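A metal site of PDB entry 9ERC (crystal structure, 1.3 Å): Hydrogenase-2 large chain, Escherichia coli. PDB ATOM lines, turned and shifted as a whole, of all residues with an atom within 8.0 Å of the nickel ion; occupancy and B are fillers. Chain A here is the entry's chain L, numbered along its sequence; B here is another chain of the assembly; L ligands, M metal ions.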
ATOM      1  N   GLU A  14     -15.243   9.595   9.659  1.00  0.00           N
ATOM      2  CA  GLU A  14     -16.033   9.367  10.866  1.00  0.00           C
ATOM      3  C   GLU A  14     -16.364   7.882  10.914  1.00  0.00           C
ATOM      4  O   GLU A  14     -16.921   7.334   9.940  1.00  0.00           O
ATOM      5  CB  GLU A  14     -17.291  10.209  10.871  1.00  0.00           C
ATOM      6  CG  GLU A  14     -18.046  10.167  12.191  1.00  0.00           C
ATOM      7  CD  GLU A  14     -18.649   8.828  12.579  1.00  0.00           C
ATOM      8  OE1 GLU A  14     -19.112   8.149  11.662  1.00  0.00           O
ATOM      9  OE2 GLU A  14     -18.637   8.448  13.809  1.00  0.00           O
ATOM     10  N   GLN A  58     -30.369  12.829  16.537  1.00  0.00           N
ATOM     11  CA  GLN A  58     -29.234  13.699  16.244  1.00  0.00           C
ATOM     12  C   GLN A  58     -27.933  12.966  16.558  1.00  0.00           C
ATOM     13  O   GLN A  58     -26.913  13.173  15.885  1.00  0.00           O
ATOM     14  CB  GLN A  58     -29.271  14.986  17.071  1.00  0.00           C
ATOM     15  CG  GLN A  58     -28.229  15.986  16.604  1.00  0.00           C
ATOM     16  CD  GLN A  58     -28.280  17.382  17.137  1.00  0.00           C
ATOM     17  OE1 GLN A  58     -27.656  18.276  16.552  1.00  0.00           O
ATOM     18  NE2 GLN A  58     -28.923  17.561  18.290  1.00  0.00           N
ATOM     19  N   ILE A  60     -27.079  10.077  15.908  1.00  0.00           N
ATOM     20  CA  ILE A  60     -26.542   9.242  14.848  1.00  0.00           C
ATOM     21  C   ILE A  60     -25.126   9.685  14.519  1.00  0.00           C
ATOM     22  O   ILE A  60     -24.251   8.837  14.271  1.00  0.00           O
ATOM     23  CB  ILE A  60     -27.478   9.240  13.622  1.00  0.00           C
ATOM     24  CG1 ILE A  60     -28.708   8.394  13.941  1.00  0.00           C
ATOM     25  CG2 ILE A  60     -26.739   8.779  12.375  1.00  0.00           C
ATOM     26  CD1 ILE A  60     -29.781   8.497  12.889  1.00  0.00           C
ATOM     27  N   CYS A  61     -24.892  11.002  14.524  1.00  0.00           N
ATOM     28  CA  CYS A  61     -23.570  11.460  14.145  1.00  0.00           C
ATOM     29  C   CYS A  61     -23.257  12.832  14.757  1.00  0.00           C
ATOM     30  O   CYS A  61     -24.098  13.732  14.701  1.00  0.00           O
ATOM     31  CB  CYS A  61     -23.467  11.500  12.629  1.00  0.00           C
ATOM     32  SG  CYS A  61     -21.806  11.905  12.026  1.00  0.00           S
ATOM     33  N   GLY A  62     -22.026  12.958  15.262  1.00  0.00           N
ATOM     34  CA  GLY A  62     -21.573  14.219  15.807  1.00  0.00           C
ATOM     35  C   GLY A  62     -20.647  14.979  14.871  1.00  0.00           C
ATOM     36  O   GLY A  62     -20.293  16.104  15.194  1.00  0.00           O
ATOM     37  N   VAL A  63     -20.222  14.347  13.774  1.00  0.00           N
ATOM     38  CA  VAL A  63     -19.503  15.081  12.746  1.00  0.00           C
ATOM     39  C   VAL A  63     -20.532  15.894  11.971  1.00  0.00           C
ATOM     40  O   VAL A  63     -20.489  17.110  11.965  1.00  0.00           O
ATOM     41  CB  VAL A  63     -18.684  14.145  11.860  1.00  0.00           C
ATOM     42  CG1 VAL A  63     -18.084  14.901  10.684  1.00  0.00           C
ATOM     43  CG2 VAL A  63     -17.611  13.451  12.676  1.00  0.00           C
ATOM     44  N   CYS A  64     -21.533  15.236  11.387  1.00  0.00           N
ATOM     45  CA  CYS A  64     -22.662  15.912  10.789  1.00  0.00           C
ATOM     46  C   CYS A  64     -23.742  16.112  11.845  1.00  0.00           C
ATOM     47  O   CYS A  64     -24.943  15.811  11.673  1.00  0.00           O
ATOM     48  CB  CYS A  64     -23.198  15.241   9.530  1.00  0.00           C
ATOM     49  SG  CYS A  64     -23.834  13.560   9.801  1.00  0.00           S
ATOM     50  N   THR A  65     -23.309  16.708  12.942  1.00  0.00           N
ATOM     51  CA  THR A  65     -24.262  17.218  13.920  1.00  0.00           C
ATOM     52  C   THR A  65     -25.185  18.218  13.212  1.00  0.00           C
ATOM     53  O   THR A  65     -24.854  18.715  12.145  1.00  0.00           O
ATOM     54  CB  THR A  65     -23.540  17.720  15.171  1.00  0.00           C
ATOM     55  OG1 THR A  65     -24.531  17.967  16.172  1.00  0.00           O
ATOM     56  CG2 THR A  65     -22.733  18.976  14.941  1.00  0.00           C
ATOM     57  N   THR A  67     -27.657  17.687  11.388  1.00  0.00           N
ATOM     58  CA  THR A  67     -28.369  17.235  10.193  1.00  0.00           C
ATOM     59  C   THR A  67     -29.531  16.305  10.527  1.00  0.00           C
ATOM     60  O   THR A  67     -30.619  16.429   9.971  1.00  0.00           O
ATOM     61  CB  THR A  67     -27.421  16.581   9.192  1.00  0.00           C
ATOM     62  OG1 THR A  67     -26.836  15.386   9.732  1.00  0.00           O
ATOM     63  CG2 THR A  67     -26.329  17.556   8.784  1.00  0.00           C
ATOM     64  N   HIS A  68     -29.284  15.315  11.373  1.00  0.00           N
ATOM     65  CA  HIS A  68     -30.320  14.351  11.740  1.00  0.00           C
ATOM     66  C   HIS A  68     -31.381  14.996  12.632  1.00  0.00           C
ATOM     67  O   HIS A  68     -32.538  14.592  12.591  1.00  0.00           O
ATOM     68  CB  HIS A  68     -29.679  13.146  12.425  1.00  0.00           C
ATOM     69  CG  HIS A  68     -28.821  12.356  11.523  1.00  0.00           C
ATOM     70  ND1 HIS A  68     -29.364  11.506  10.570  1.00  0.00           N
ATOM     71  CD2 HIS A  68     -27.486  12.307  11.381  1.00  0.00           C
ATOM     72  CE1 HIS A  68     -28.372  10.981   9.868  1.00  0.00           C
ATOM     73  NE2 HIS A  68     -27.202  11.434  10.340  1.00  0.00           N
ATOM     74  N   HIS A  99     -22.812  25.029   9.949  1.00  0.00           N
ATOM     75  CA  HIS A  99     -22.303  23.710  10.281  1.00  0.00           C
ATOM     76  C   HIS A  99     -21.541  23.125   9.076  1.00  0.00           C
ATOM     77  O   HIS A  99     -20.444  22.597   9.212  1.00  0.00           O
ATOM     78  CB  HIS A  99     -23.441  22.729  10.622  1.00  0.00           C
ATOM     79  CG  HIS A  99     -22.840  21.379  10.712  1.00  0.00           C
ATOM     80  ND1 HIS A  99     -22.082  20.972  11.795  1.00  0.00           N
ATOM     81  CD2 HIS A  99     -22.724  20.437   9.770  1.00  0.00           C
ATOM     82  CE1 HIS A  99     -21.556  19.808  11.495  1.00  0.00           C
ATOM     83  NE2 HIS A  99     -21.914  19.461  10.275  1.00  0.00           N
ATOM     84  N   ASP A 103     -17.813  21.649   8.520  1.00  0.00           N
ATOM     85  CA  ASP A 103     -17.667  20.243   8.187  1.00  0.00           C
ATOM     86  C   ASP A 103     -16.760  20.093   6.965  1.00  0.00           C
ATOM     87  O   ASP A 103     -15.788  19.347   6.987  1.00  0.00           O
ATOM     88  CB  ASP A 103     -19.091  19.703   7.999  1.00  0.00           C
ATOM     89  CG  ASP A 103     -19.244  18.199   8.079  1.00  0.00           C
ATOM     90  OD1 ASP A 103     -18.278  17.516   7.668  1.00  0.00           O
ATOM     91  OD2 ASP A 103     -20.323  17.736   8.488  1.00  0.00           O
ATOM     92  N   ALA A 477     -27.498  17.256   3.213  1.00  0.00           N
ATOM     93  CA  ALA A 477     -26.473  17.239   4.242  1.00  0.00           C
ATOM     94  C   ALA A 477     -25.110  17.443   3.586  1.00  0.00           C
ATOM     95  O   ALA A 477     -24.977  17.327   2.364  1.00  0.00           O
ATOM     96  CB  ALA A 477     -26.559  15.947   5.026  1.00  0.00           C
ATOM     97  N   PRO A 478     -24.043  17.631   4.385  1.00  0.00           N
ATOM     98  CA  PRO A 478     -22.700  17.801   3.830  1.00  0.00           C
ATOM     99  C   PRO A 478     -22.236  16.647   2.946  1.00  0.00           C
ATOM    100  O   PRO A 478     -21.528  16.872   1.980  1.00  0.00           O
ATOM    101  CB  PRO A 478     -21.801  17.893   5.091  1.00  0.00           C
ATOM    102  CG  PRO A 478     -22.707  18.524   6.127  1.00  0.00           C
ATOM    103  CD  PRO A 478     -24.072  17.918   5.847  1.00  0.00           C
ATOM    104  N   ARG A 479     -22.735  15.434   3.247  1.00  0.00           N
ATOM    105  CA  ARG A 479     -22.354  14.260   2.478  1.00  0.00           C
ATOM    106  C   ARG A 479     -23.437  13.831   1.509  1.00  0.00           C
ATOM    107  O   ARG A 479     -23.228  12.848   0.814  1.00  0.00           O
ATOM    108  CB  ARG A 479     -22.033  13.123   3.443  1.00  0.00           C
ATOM    109  CG  ARG A 479     -20.731  13.385   4.202  1.00  0.00           C
ATOM    110  CD  ARG A 479     -20.524  12.642   5.502  1.00  0.00           C
ATOM    111  NE  ARG A 479     -19.329  13.091   6.208  1.00  0.00           N
ATOM    112  CZ  ARG A 479     -19.247  14.239   6.891  1.00  0.00           C
ATOM    113  NH1 ARG A 479     -20.339  14.923   7.198  1.00  0.00           N
ATOM    114  NH2 ARG A 479     -18.074  14.697   7.279  1.00  0.00           N
ATOM    115  N   VAL A 500     -29.337   7.474   4.881  1.00  0.00           N
ATOM    116  CA  VAL A 500     -28.374   8.524   5.150  1.00  0.00           C
ATOM    117  C   VAL A 500     -27.422   8.616   3.966  1.00  0.00           C
ATOM    118  O   VAL A 500     -27.205   7.641   3.251  1.00  0.00           O
ATOM    119  CB  VAL A 500     -27.684   8.215   6.491  1.00  0.00           C
ATOM    120  CG1 VAL A 500     -26.750   9.311   6.955  1.00  0.00           C
ATOM    121  CG2 VAL A 500     -28.710   7.922   7.579  1.00  0.00           C
ATOM    122  N   PRO A 501     -26.823   9.783   3.637  1.00  0.00           N
ATOM    123  CA  PRO A 501     -26.037   9.860   2.420  1.00  0.00           C
ATOM    124  C   PRO A 501     -24.905   8.842   2.330  1.00  0.00           C
ATOM    125  O   PRO A 501     -24.712   8.214   1.271  1.00  0.00           O
ATOM    126  CB  PRO A 501     -25.525  11.322   2.364  1.00  0.00           C
ATOM    127  CG  PRO A 501     -25.881  11.899   3.695  1.00  0.00           C
ATOM    128  CD  PRO A 501     -27.060  11.098   4.232  1.00  0.00           C
ATOM    129  N   SER A 502     -24.159   8.625   3.418  1.00  0.00           N
ATOM    130  CA  SER A 502     -23.117   7.604   3.364  1.00  0.00           C
ATOM    131  C   SER A 502     -23.691   6.195   3.209  1.00  0.00           C
ATOM    132  O   SER A 502     -22.966   5.320   2.736  1.00  0.00           O
ATOM    133  CB  SER A 502     -22.200   7.693   4.553  1.00  0.00           C
ATOM    134  OG  SER A 502     -21.389   8.869   4.465  1.00  0.00           O
ATOM    135  N   ASP A 544     -15.984  11.498   1.696  1.00  0.00           N
ATOM    136  CA  ASP A 544     -16.216  11.978   3.052  1.00  0.00           C
ATOM    137  C   ASP A 544     -17.039  10.956   3.848  1.00  0.00           C
ATOM    138  O   ASP A 544     -18.129  11.220   4.378  1.00  0.00           O
ATOM    139  CB  ASP A 544     -16.820  13.359   2.969  1.00  0.00           C
ATOM    140  CG  ASP A 544     -16.979  14.113   4.268  1.00  0.00           C
ATOM    141  OD1 ASP A 544     -16.442  13.657   5.310  1.00  0.00           O
ATOM    142  OD2 ASP A 544     -17.703  15.153   4.186  1.00  0.00           O
ATOM    143  N   PRO A 545     -16.516   9.709   3.979  1.00  0.00           N
ATOM    144  CA  PRO A 545     -17.288   8.672   4.674  1.00  0.00           C
ATOM    145  C   PRO A 545     -17.666   9.036   6.106  1.00  0.00           C
ATOM    146  O   PRO A 545     -16.836   9.506   6.880  1.00  0.00           O
ATOM    147  CB  PRO A 545     -16.406   7.445   4.653  1.00  0.00           C
ATOM    148  CG  PRO A 545     -15.454   7.690   3.503  1.00  0.00           C
ATOM    149  CD  PRO A 545     -15.226   9.190   3.501  1.00  0.00           C
ATOM    150  N   CYS A 546     -18.917   8.707   6.452  1.00  0.00           N
ATOM    151  CA  CYS A 546     -19.355   8.842   7.821  1.00  0.00           C
ATOM    152  C   CYS A 546     -20.118   7.549   8.159  1.00  0.00           C
ATOM    153  O   CYS A 546     -21.233   7.376   7.672  1.00  0.00           O
ATOM    154  CB  CYS A 546     -20.187  10.092   7.916  1.00  0.00           C
ATOM    155  SG  CYS A 546     -20.662  10.431   9.640  1.00  0.00           S
ATOM    156  N   MET A 547     -19.490   6.670   8.937  1.00  0.00           N
ATOM    157  CA  MET A 547     -20.041   5.328   9.081  1.00  0.00           C
ATOM    158  C   MET A 547     -21.031   5.237  10.226  1.00  0.00           C
ATOM    159  O   MET A 547     -21.890   4.341  10.235  1.00  0.00           O
ATOM    160  CB  MET A 547     -18.921   4.290   9.224  1.00  0.00           C
ATOM    161  CG  MET A 547     -17.977   4.260   8.020  1.00  0.00           C
ATOM    162  SD  MET A 547     -18.756   4.303   6.394  1.00  0.00           S
ATOM    163  CE  MET A 547     -19.571   2.714   6.433  1.00  0.00           C
ATOM    164  N   ALA A 548     -20.958   6.149  11.196  1.00  0.00           N
ATOM    165  CA  ALA A 548     -22.021   6.277  12.186  1.00  0.00           C
ATOM    166  C   ALA A 548     -23.315   6.655  11.467  1.00  0.00           C
ATOM    167  O   ALA A 548     -24.402   6.126  11.712  1.00  0.00           O
ATOM    168  CB  ALA A 548     -21.609   7.295  13.249  1.00  0.00           C
ATOM    169  N   CYS A 549     -23.172   7.594  10.538  1.00  0.00           N
ATOM    170  CA  CYS A 549     -24.260   7.926   9.619  1.00  0.00           C
ATOM    171  C   CYS A 549     -24.710   6.741   8.774  1.00  0.00           C
ATOM    172  O   CYS A 549     -25.904   6.494   8.627  1.00  0.00           O
ATOM    173  CB  CYS A 549     -23.824   9.041   8.699  1.00  0.00           C
ATOM    174  SG  CYS A 549     -24.231  10.666   9.424  1.00  0.00           S
ATOM    175  N   ALA A 550     -23.762   6.070   8.110  1.00  0.00           N
ATOM    176  CA  ALA A 550     -24.162   5.069   7.125  1.00  0.00           C
ATOM    177  C   ALA A 550     -24.986   3.971   7.776  1.00  0.00           C
ATOM    178  O   ALA A 550     -25.880   3.446   7.139  1.00  0.00           O
ATOM    179  CB  ALA A 550     -22.952   4.496   6.457  1.00  0.00           C
ATOM    180  N   CYS B  21     -20.415   8.515  18.179  1.00  0.00           N
ATOM    181  CA  CYS B  21     -20.944   9.282  17.067  1.00  0.00           C
ATOM    182  C   CYS B  21     -19.890  10.281  16.553  1.00  0.00           C
ATOM    183  O   CYS B  21     -20.117  10.929  15.527  1.00  0.00           O
ATOM    184  CB  CYS B  21     -22.228  10.020  17.414  1.00  0.00           C
ATOM    185  SG  CYS B  21     -21.944  11.531  18.398  1.00  0.00           S
ATOM    186  N   THR B  22     -18.773  10.387  17.273  1.00  0.00           N
ATOM    187  CA  THR B  22     -17.617  11.244  16.998  1.00  0.00           C
ATOM    188  C   THR B  22     -17.831  12.639  17.584  1.00  0.00           C
ATOM    189  O   THR B  22     -16.924  13.469  17.560  1.00  0.00           O
ATOM    190  CB  THR B  22     -17.177  11.222  15.535  1.00  0.00           C
ATOM    191  OG1 THR B  22     -17.051   9.843  15.175  1.00  0.00           O
ATOM    192  CG2 THR B  22     -15.850  11.900  15.277  1.00  0.00           C
HETATM  193 FE1  LIG L   1     -23.930  12.371   7.899  1.00  0.00          FE
HETATM  194  C1  LIG L   1     -23.553  11.159   6.532  1.00  0.00           C
HETATM  195  N1  LIG L   1     -23.377  10.429   5.692  1.00  0.00           N
HETATM  196  C2  LIG L   1     -23.523  13.828   6.837  1.00  0.00           C
HETATM  197  N2  LIG L   1     -23.312  14.707   6.154  1.00  0.00           N
HETATM  198  C3  LIG L   1     -25.608  12.617   7.387  1.00  0.00           C
HETATM  199  O1  LIG L   1     -26.710  12.799   7.133  1.00  0.00           O
HETATM  200 NI    NI M   1     -22.244  11.920   9.841  1.00  0.00          NI
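Of the 27 residues printed, 4 come within 4 Å of the nickel ion.
The nearest printed residue that does not touch the nickel ion is Arg 479 (4.4 Å).
The side-chain sulfur (SG) of Cys 546 binds the nickel ion (2.2 Å).
SG of Cys 61 binds the nickel ion.
SG of Cys 64 is bound to the nickel ion, 2.3 Å away.
SG of Cys 549 binds the nickel ion, 2.4 Å away.
The side-chain sulfur (SG) of Cys 546 lies close to the side-chain carboxylate (OE1) of Glu 14 (3.4 Å).
The side-chain sulfur of Cys 549 lies close to a ring nitrogen (NE2) of His 68.
The side-chain hydroxyl (OG) of Ser 502 is in hydrogen-bond range of the backbone NH (N) of Cys 546 (3.2 Å).
The side-chain hydroxyl of Thr 67 lies within hydrogen-bond range of the backbone carbonyl oxygen of Cys 64 (2.7 Å).
The side-chain sulfur of Cys 61 sits close to the backbone NH of Val 63.
A nitrogen (N1) of the ligand lies within hydrogen-bond range of the backbone NH (N) of Ser 502 (3.0 Å).
The guanidinium group of Arg 479 lies within hydrogen-bond range of a nitrogen (N2) of the ligand.
SG of Cys 549 is bound to FE1 of the ligand (2.3 Å).
The backbone NH (N) of Arg 479 sits at hydrogen-bond distance from a nitrogen (N2) of the ligand.
The side-chain hydroxyl (OG) of Ser 502 sits at hydrogen-bond distance from a nitrogen (N1) of the ligand.
The side-chain sulfur of Cys 64 binds an iron atom (FE1) of the ligand, 2.2 Å away.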
